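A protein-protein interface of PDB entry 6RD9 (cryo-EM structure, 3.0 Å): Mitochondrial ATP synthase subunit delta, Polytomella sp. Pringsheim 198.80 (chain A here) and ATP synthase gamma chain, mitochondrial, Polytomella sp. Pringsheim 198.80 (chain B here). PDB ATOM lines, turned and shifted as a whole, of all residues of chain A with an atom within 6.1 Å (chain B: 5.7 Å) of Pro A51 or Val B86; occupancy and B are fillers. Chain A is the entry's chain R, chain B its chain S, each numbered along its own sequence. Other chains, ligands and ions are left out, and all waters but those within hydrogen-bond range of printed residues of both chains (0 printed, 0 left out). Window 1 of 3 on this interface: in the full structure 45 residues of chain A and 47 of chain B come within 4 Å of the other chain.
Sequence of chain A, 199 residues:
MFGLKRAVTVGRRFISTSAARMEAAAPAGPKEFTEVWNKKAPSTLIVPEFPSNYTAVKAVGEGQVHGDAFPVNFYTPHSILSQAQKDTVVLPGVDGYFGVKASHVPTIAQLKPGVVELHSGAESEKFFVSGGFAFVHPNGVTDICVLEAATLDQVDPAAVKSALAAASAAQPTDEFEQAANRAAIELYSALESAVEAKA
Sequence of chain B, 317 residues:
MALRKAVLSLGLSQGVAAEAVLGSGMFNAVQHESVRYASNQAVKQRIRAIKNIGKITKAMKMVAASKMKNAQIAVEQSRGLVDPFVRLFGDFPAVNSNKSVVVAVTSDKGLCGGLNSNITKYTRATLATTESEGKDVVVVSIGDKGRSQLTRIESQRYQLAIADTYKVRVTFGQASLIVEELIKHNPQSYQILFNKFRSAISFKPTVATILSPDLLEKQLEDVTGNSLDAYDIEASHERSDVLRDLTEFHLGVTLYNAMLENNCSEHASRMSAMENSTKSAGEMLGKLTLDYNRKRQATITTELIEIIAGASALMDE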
ATOM      1  N   GLU A  49     -25.184 -18.357   2.236  1.00  0.00           N
ATOM      2  CA  GLU A  49     -24.072 -18.052   3.108  1.00  0.00           C
ATOM      3  C   GLU A  49     -23.498 -16.688   2.753  1.00  0.00           C
ATOM      4  O   GLU A  49     -23.842 -16.082   1.738  1.00  0.00           O
ATOM      5  CB  GLU A  49     -23.004 -19.126   3.006  1.00  0.00           C
ATOM      6  CG  GLU A  49     -23.467 -20.472   3.482  1.00  0.00           C
ATOM      7  CD  GLU A  49     -23.573 -20.567   4.982  1.00  0.00           C
ATOM      8  OE1 GLU A  49     -22.826 -19.860   5.685  1.00  0.00           O
ATOM      9  OE2 GLU A  49     -24.418 -21.348   5.463  1.00  0.00           O
ATOM     10  N   PHE A  50     -22.634 -16.191   3.626  1.00  0.00           N
ATOM     11  CA  PHE A  50     -21.999 -14.896   3.470  1.00  0.00           C
ATOM     12  C   PHE A  50     -20.518 -15.036   3.767  1.00  0.00           C
ATOM     13  O   PHE A  50     -20.123 -15.929   4.521  1.00  0.00           O
ATOM     14  CB  PHE A  50     -22.627 -13.865   4.411  1.00  0.00           C
ATOM     15  CG  PHE A  50     -24.113 -13.891   4.414  1.00  0.00           C
ATOM     16  CD1 PHE A  50     -24.801 -14.507   5.439  1.00  0.00           C
ATOM     17  CD2 PHE A  50     -24.824 -13.309   3.385  1.00  0.00           C
ATOM     18  CE1 PHE A  50     -26.173 -14.539   5.439  1.00  0.00           C
ATOM     19  CE2 PHE A  50     -26.193 -13.335   3.382  1.00  0.00           C
ATOM     20  CZ  PHE A  50     -26.867 -13.956   4.410  1.00  0.00           C
ATOM     21  N   PRO A  51     -19.672 -14.181   3.184  1.00  0.00           N
ATOM     22  CA  PRO A  51     -18.228 -14.277   3.457  1.00  0.00           C
ATOM     23  C   PRO A  51     -17.827 -13.946   4.889  1.00  0.00           C
ATOM     24  O   PRO A  51     -16.680 -14.223   5.261  1.00  0.00           O
ATOM     25  CB  PRO A  51     -17.616 -13.284   2.467  1.00  0.00           C
ATOM     26  CG  PRO A  51     -18.754 -12.467   1.962  1.00  0.00           C
ATOM     27  CD  PRO A  51     -19.952 -13.313   2.030  1.00  0.00           C
ATOM     28  N   SER A  52     -18.723 -13.397   5.712  1.00  0.00           N
ATOM     29  CA  SER A  52     -18.432 -13.259   7.132  1.00  0.00           C
ATOM     30  C   SER A  52     -18.470 -14.585   7.869  1.00  0.00           C
ATOM     31  O   SER A  52     -17.937 -14.676   8.978  1.00  0.00           O
ATOM     32  CB  SER A  52     -19.418 -12.299   7.783  1.00  0.00           C
ATOM     33  OG  SER A  52     -19.168 -10.988   7.350  1.00  0.00           O
ATOM     34  N   ASN A  53     -19.088 -15.606   7.292  1.00  0.00           N
ATOM     35  CA  ASN A  53     -19.186 -16.898   7.949  1.00  0.00           C
ATOM     36  C   ASN A  53     -17.955 -17.759   7.724  1.00  0.00           C
ATOM     37  O   ASN A  53     -17.900 -18.879   8.237  1.00  0.00           O
ATOM     38  CB  ASN A  53     -20.434 -17.631   7.465  1.00  0.00           C
ATOM     39  CG  ASN A  53     -21.649 -16.734   7.427  1.00  0.00           C
ATOM     40  OD1 ASN A  53     -22.326 -16.630   6.409  1.00  0.00           O
ATOM     41  ND2 ASN A  53     -21.921 -16.065   8.535  1.00  0.00           N
ATOM     42  N   TYR A  54     -16.969 -17.268   6.982  1.00  0.00           N
ATOM     43  CA  TYR A  54     -15.787 -18.051   6.671  1.00  0.00           C
ATOM     44  C   TYR A  54     -14.503 -17.457   7.221  1.00  0.00           C
ATOM     45  O   TYR A  54     -13.462 -18.114   7.163  1.00  0.00           O
ATOM     46  CB  TYR A  54     -15.670 -18.229   5.161  1.00  0.00           C
ATOM     47  CG  TYR A  54     -16.897 -18.876   4.589  1.00  0.00           C
ATOM     48  CD1 TYR A  54     -17.129 -20.227   4.785  1.00  0.00           C
ATOM     49  CD2 TYR A  54     -17.834 -18.139   3.878  1.00  0.00           C
ATOM     50  CE1 TYR A  54     -18.246 -20.827   4.283  1.00  0.00           C
ATOM     51  CE2 TYR A  54     -18.960 -18.742   3.367  1.00  0.00           C
ATOM     52  CZ  TYR A  54     -19.150 -20.088   3.577  1.00  0.00           C
ATOM     53  OH  TYR A  54     -20.243 -20.733   3.087  1.00  0.00           O
ATOM     54  N   THR A  55     -14.540 -16.249   7.755  1.00  0.00           N
ATOM     55  CA  THR A  55     -13.382 -15.687   8.429  1.00  0.00           C
ATOM     56  C   THR A  55     -13.674 -15.548   9.917  1.00  0.00           C
ATOM     57  O   THR A  55     -14.762 -15.123  10.317  1.00  0.00           O
ATOM     58  CB  THR A  55     -12.971 -14.346   7.811  1.00  0.00           C
ATOM     59  OG1 THR A  55     -11.968 -13.727   8.620  1.00  0.00           O
ATOM     60  CG2 THR A  55     -14.158 -13.418   7.654  1.00  0.00           C
ATOM     61  N   VAL B  82     -10.145 -12.609  -0.007  1.00  0.00           N
ATOM     62  CA  VAL B  82     -11.473 -12.060   0.257  1.00  0.00           C
ATOM     63  C   VAL B  82     -11.671 -11.714   1.720  1.00  0.00           C
ATOM     64  O   VAL B  82     -12.594 -10.965   2.041  1.00  0.00           O
ATOM     65  CB  VAL B  82     -12.597 -13.014  -0.190  1.00  0.00           C
ATOM     66  CG1 VAL B  82     -12.382 -13.443  -1.612  1.00  0.00           C
ATOM     67  CG2 VAL B  82     -12.690 -14.218   0.709  1.00  0.00           C
ATOM     68  N   ASP B  83     -10.813 -12.211   2.608  1.00  0.00           N
ATOM     69  CA  ASP B  83     -10.947 -12.012   4.047  1.00  0.00           C
ATOM     70  C   ASP B  83     -10.645 -10.587   4.529  1.00  0.00           C
ATOM     71  O   ASP B  83     -11.392 -10.102   5.384  1.00  0.00           O
ATOM     72  CB  ASP B  83     -10.069 -13.021   4.797  1.00  0.00           C
ATOM     73  CG  ASP B  83     -10.574 -14.438   4.678  1.00  0.00           C
ATOM     74  OD1 ASP B  83     -11.807 -14.626   4.610  1.00  0.00           O
ATOM     75  OD2 ASP B  83      -9.740 -15.369   4.643  1.00  0.00           O
ATOM     76  N   PRO B  84      -9.603  -9.874   4.058  1.00  0.00           N
ATOM     77  CA  PRO B  84      -9.431  -8.498   4.548  1.00  0.00           C
ATOM     78  C   PRO B  84     -10.504  -7.530   4.101  1.00  0.00           C
ATOM     79  O   PRO B  84     -10.823  -6.601   4.846  1.00  0.00           O
ATOM     80  CB  PRO B  84      -8.060  -8.103   3.994  1.00  0.00           C
ATOM     81  CG  PRO B  84      -7.836  -9.007   2.934  1.00  0.00           C
ATOM     82  CD  PRO B  84      -8.370 -10.273   3.364  1.00  0.00           C
ATOM     83  N   PHE B  85     -11.082  -7.710   2.923  1.00  0.00           N
ATOM     84  CA  PHE B  85     -12.102  -6.774   2.491  1.00  0.00           C
ATOM     85  C   PHE B  85     -13.428  -6.983   3.199  1.00  0.00           C
ATOM     86  O   PHE B  85     -14.271  -6.084   3.177  1.00  0.00           O
ATOM     87  CB  PHE B  85     -12.324  -6.888   1.001  1.00  0.00           C
ATOM     88  CG  PHE B  85     -11.145  -6.526   0.192  1.00  0.00           C
ATOM     89  CD1 PHE B  85     -10.846  -5.210  -0.056  1.00  0.00           C
ATOM     90  CD2 PHE B  85     -10.336  -7.504  -0.334  1.00  0.00           C
ATOM     91  CE1 PHE B  85      -9.758  -4.885  -0.807  1.00  0.00           C
ATOM     92  CE2 PHE B  85      -9.246  -7.176  -1.089  1.00  0.00           C
ATOM     93  CZ  PHE B  85      -8.957  -5.872  -1.320  1.00  0.00           C
ATOM     94  N   VAL B  86     -13.657  -8.149   3.798  1.00  0.00           N
ATOM     95  CA  VAL B  86     -14.878  -8.317   4.572  1.00  0.00           C
ATOM     96  C   VAL B  86     -14.680  -7.959   6.032  1.00  0.00           C
ATOM     97  O   VAL B  86     -15.665  -7.897   6.778  1.00  0.00           O
ATOM     98  CB  VAL B  86     -15.466  -9.735   4.478  1.00  0.00           C
ATOM     99  CG1 VAL B  86     -15.656 -10.136   3.036  1.00  0.00           C
ATOM    100  CG2 VAL B  86     -14.601 -10.718   5.205  1.00  0.00           C
ATOM    101  N   ARG B  87     -13.445  -7.743   6.474  1.00  0.00           N
ATOM    102  CA  ARG B  87     -13.263  -7.164   7.791  1.00  0.00           C
ATOM    103  C   ARG B  87     -12.891  -5.696   7.735  1.00  0.00           C
ATOM    104  O   ARG B  87     -12.927  -5.026   8.770  1.00  0.00           O
ATOM    105  CB  ARG B  87     -12.220  -7.935   8.605  1.00  0.00           C
ATOM    106  CG  ARG B  87     -10.885  -8.128   7.982  1.00  0.00           C
ATOM    107  CD  ARG B  87      -9.996  -8.768   9.011  1.00  0.00           C
ATOM    108  NE  ARG B  87      -8.768  -9.317   8.461  1.00  0.00           N
ATOM    109  CZ  ARG B  87      -8.575 -10.606   8.239  1.00  0.00           C
ATOM    110  NH1 ARG B  87      -9.539 -11.465   8.513  1.00  0.00           N
ATOM    111  NH2 ARG B  87      -7.427 -11.033   7.743  1.00  0.00           N
ATOM    112  N   LEU B  88     -12.555  -5.178   6.560  1.00  0.00           N
ATOM    113  CA  LEU B  88     -12.390  -3.740   6.415  1.00  0.00           C
ATOM    114  C   LEU B  88     -13.722  -3.077   6.119  1.00  0.00           C
ATOM    115  O   LEU B  88     -14.095  -2.096   6.764  1.00  0.00           O
ATOM    116  CB  LEU B  88     -11.390  -3.430   5.305  1.00  0.00           C
ATOM    117  CG  LEU B  88     -10.865  -2.006   5.267  1.00  0.00           C
ATOM    118  CD1 LEU B  88     -10.015  -1.791   6.479  1.00  0.00           C
ATOM    119  CD2 LEU B  88     -10.055  -1.783   4.025  1.00  0.00           C
ATOM    120  N   PHE B  89     -14.458  -3.615   5.155  1.00  0.00           N
ATOM    121  CA  PHE B  89     -15.714  -3.046   4.702  1.00  0.00           C
ATOM    122  C   PHE B  89     -16.925  -3.750   5.276  1.00  0.00           C
ATOM    123  O   PHE B  89     -18.048  -3.307   5.032  1.00  0.00           O
ATOM    124  CB  PHE B  89     -15.785  -3.099   3.184  1.00  0.00           C
ATOM    125  CG  PHE B  89     -14.865  -2.154   2.513  1.00  0.00           C
ATOM    126  CD1 PHE B  89     -14.519  -0.967   3.116  1.00  0.00           C
ATOM    127  CD2 PHE B  89     -14.334  -2.455   1.279  1.00  0.00           C
ATOM    128  CE1 PHE B  89     -13.664  -0.098   2.500  1.00  0.00           C
ATOM    129  CE2 PHE B  89     -13.481  -1.586   0.656  1.00  0.00           C
ATOM    130  CZ  PHE B  89     -13.151  -0.406   1.267  1.00  0.00           C
ATOM    131  N   GLY B  90     -16.733  -4.841   6.004  1.00  0.00           N
ATOM    132  CA  GLY B  90     -17.873  -5.541   6.541  1.00  0.00           C
ATOM    133  C   GLY B  90     -18.616  -6.353   5.490  1.00  0.00           C
ATOM    134  O   GLY B  90     -18.091  -6.712   4.436  1.00  0.00           O
ATOM    135  N   ASP B  91     -19.878  -6.632   5.804  1.00  0.00           N
ATOM    136  CA  ASP B  91     -20.724  -7.484   4.973  1.00  0.00           C
ATOM    137  C   ASP B  91     -22.153  -6.991   5.109  1.00  0.00           C
ATOM    138  O   ASP B  91     -22.779  -7.204   6.149  1.00  0.00           O
ATOM    139  CB  ASP B  91     -20.626  -8.927   5.421  1.00  0.00           C
ATOM    140  CG  ASP B  91     -20.887  -9.903   4.318  1.00  0.00           C
ATOM    141  OD1 ASP B  91     -20.371 -11.029   4.428  1.00  0.00           O
ATOM    142  OD2 ASP B  91     -21.595  -9.556   3.351  1.00  0.00           O
ATOM    143  N   THR B 206     -23.518 -18.596  -1.897  1.00  0.00           N
ATOM    144  CA  THR B 206     -23.104 -17.393  -1.210  1.00  0.00           C
ATOM    145  C   THR B 206     -23.632 -16.187  -1.963  1.00  0.00           C
ATOM    146  O   THR B 206     -23.708 -16.197  -3.194  1.00  0.00           O
ATOM    147  CB  THR B 206     -21.583 -17.337  -1.107  1.00  0.00           C
ATOM    148  OG1 THR B 206     -21.102 -18.590  -0.623  1.00  0.00           O
ATOM    149  CG2 THR B 206     -21.132 -16.267  -0.142  1.00  0.00           C
ATOM    150  N   VAL B 207     -24.049 -15.177  -1.212  1.00  0.00           N
ATOM    151  CA  VAL B 207     -24.213 -13.828  -1.722  1.00  0.00           C
ATOM    152  C   VAL B 207     -23.086 -12.990  -1.148  1.00  0.00           C
ATOM    153  O   VAL B 207     -22.951 -12.864   0.074  1.00  0.00           O
ATOM    154  CB  VAL B 207     -25.577 -13.240  -1.338  1.00  0.00           C
ATOM    155  CG1 VAL B 207     -25.721 -11.851  -1.903  1.00  0.00           C
ATOM    156  CG2 VAL B 207     -26.672 -14.130  -1.810  1.00  0.00           C
ATOM    157  N   ALA B 208     -22.280 -12.411  -2.025  1.00  0.00           N
ATOM    158  CA  ALA B 208     -21.176 -11.565  -1.609  1.00  0.00           C
ATOM    159  C   ALA B 208     -21.442 -10.184  -2.160  1.00  0.00           C
ATOM    160  O   ALA B 208     -21.625 -10.020  -3.367  1.00  0.00           O
ATOM    161  CB  ALA B 208     -19.837 -12.096  -2.106  1.00  0.00           C
ATOM    162  N   THR B 209     -21.476  -9.202  -1.278  1.00  0.00           N
ATOM    163  CA  THR B 209     -21.944  -7.868  -1.600  1.00  0.00           C
ATOM    164  C   THR B 209     -20.828  -6.842  -1.468  1.00  0.00           C
ATOM    165  O   THR B 209     -20.010  -6.908  -0.547  1.00  0.00           O
ATOM    166  CB  THR B 209     -23.119  -7.518  -0.714  1.00  0.00           C
ATOM    167  OG1 THR B 209     -23.383  -6.115  -0.788  1.00  0.00           O
ATOM    168  CG2 THR B 209     -22.829  -7.947   0.697  1.00  0.00           C
ATOM    169  N   HIS B 250     -11.957  -4.712  -4.420  1.00  0.00           N
ATOM    170  CA  HIS B 250     -12.807  -5.642  -3.689  1.00  0.00           C
ATOM    171  C   HIS B 250     -13.813  -6.299  -4.613  1.00  0.00           C
ATOM    172  O   HIS B 250     -14.251  -7.422  -4.356  1.00  0.00           O
ATOM    173  CB  HIS B 250     -13.499  -4.923  -2.540  1.00  0.00           C
ATOM    174  CG  HIS B 250     -14.505  -5.750  -1.811  1.00  0.00           C
ATOM    175  ND1 HIS B 250     -14.327  -7.091  -1.570  1.00  0.00           N
ATOM    176  CD2 HIS B 250     -15.634  -5.399  -1.155  1.00  0.00           C
ATOM    177  CE1 HIS B 250     -15.339  -7.548  -0.857  1.00  0.00           C
ATOM    178  NE2 HIS B 250     -16.147  -6.540  -0.592  1.00  0.00           N
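Thr B206 touches Glu A49 (CG2 to O, 3.3 Å). Asp B91 touches Phe A50. Phe A50 touches Thr B206 (CA to CG2, 3.96 Å). O of Val B207 touches CD2 of Phe A50 (3.8 Å). Pro A51 touches Val B86 (CB to CG1, 3.8 Å). Pro A51 touches Thr B206 (CD to CG2, 3.9 Å). CD of Pro A51 touches O of Val B207 (3.6 Å). CB of Thr A55 touches OD1 of Asp B83, at 3.4 Å. CG2 of Thr A55 touches CG2 of Val B86 (3.7 Å).
NH1 of Arg B87 sits at hydrogen-bond distance from OG1 of Thr A55, at 3.3 Å. OD1 of Asp B91 sits close to N of Pro A51 (3.5 Å). O of Glu A49 is in hydrogen-bond range of N of Val B207 (3.1 Å). N of Ser A52 is in hydrogen-bond range of OD1 of Asp B91 (3.2 Å).
Of the 7 printed residues of chain A, 5 touch a printed residue of chain B. Hydrophobic or aromatic side chains of chain A that line the printed part of chain B: Phe A50 and Pro A51. Among the printed residues, 13 pairs touch across the chains.
The side-chain amide oxygen (OD1) of Asn A53 lies close to the side-chain carboxylate (OE1) of Glu A49 (3.3 Å). N of Phe A50 sits at hydrogen-bond distance from OD1 of Asn A53, 2.8 Å away.
Of chain B, only Val B86 (3.8 Å), Asp B91 (3.3 Å), Thr B206 (3.9 Å) and Val B207 (3.6 Å) come within 4 Å of Pro A51. Printed residues of chain A within 4 Å of Val B86: Pro A51 (3.8 Å) and Thr A55 (3.7 Å). Of the printed residues of chain A, Asp B91 touches Phe A50 (3.6 Å), Pro A51 (3.3 Å) and Ser A52 (3.2 Å). Of the printed residues of chain A, Thr B206 touches Glu A49 (3.3 Å), Phe A50 (3.96 Å) and Pro A51 (3.9 Å). The nearest residue of chain A that does not touch Val B86 is Ser A52 (4.7 Å). The nearest printed residue of chain B that does not touch Phe A50 is Ala B208 (6.0 Å).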
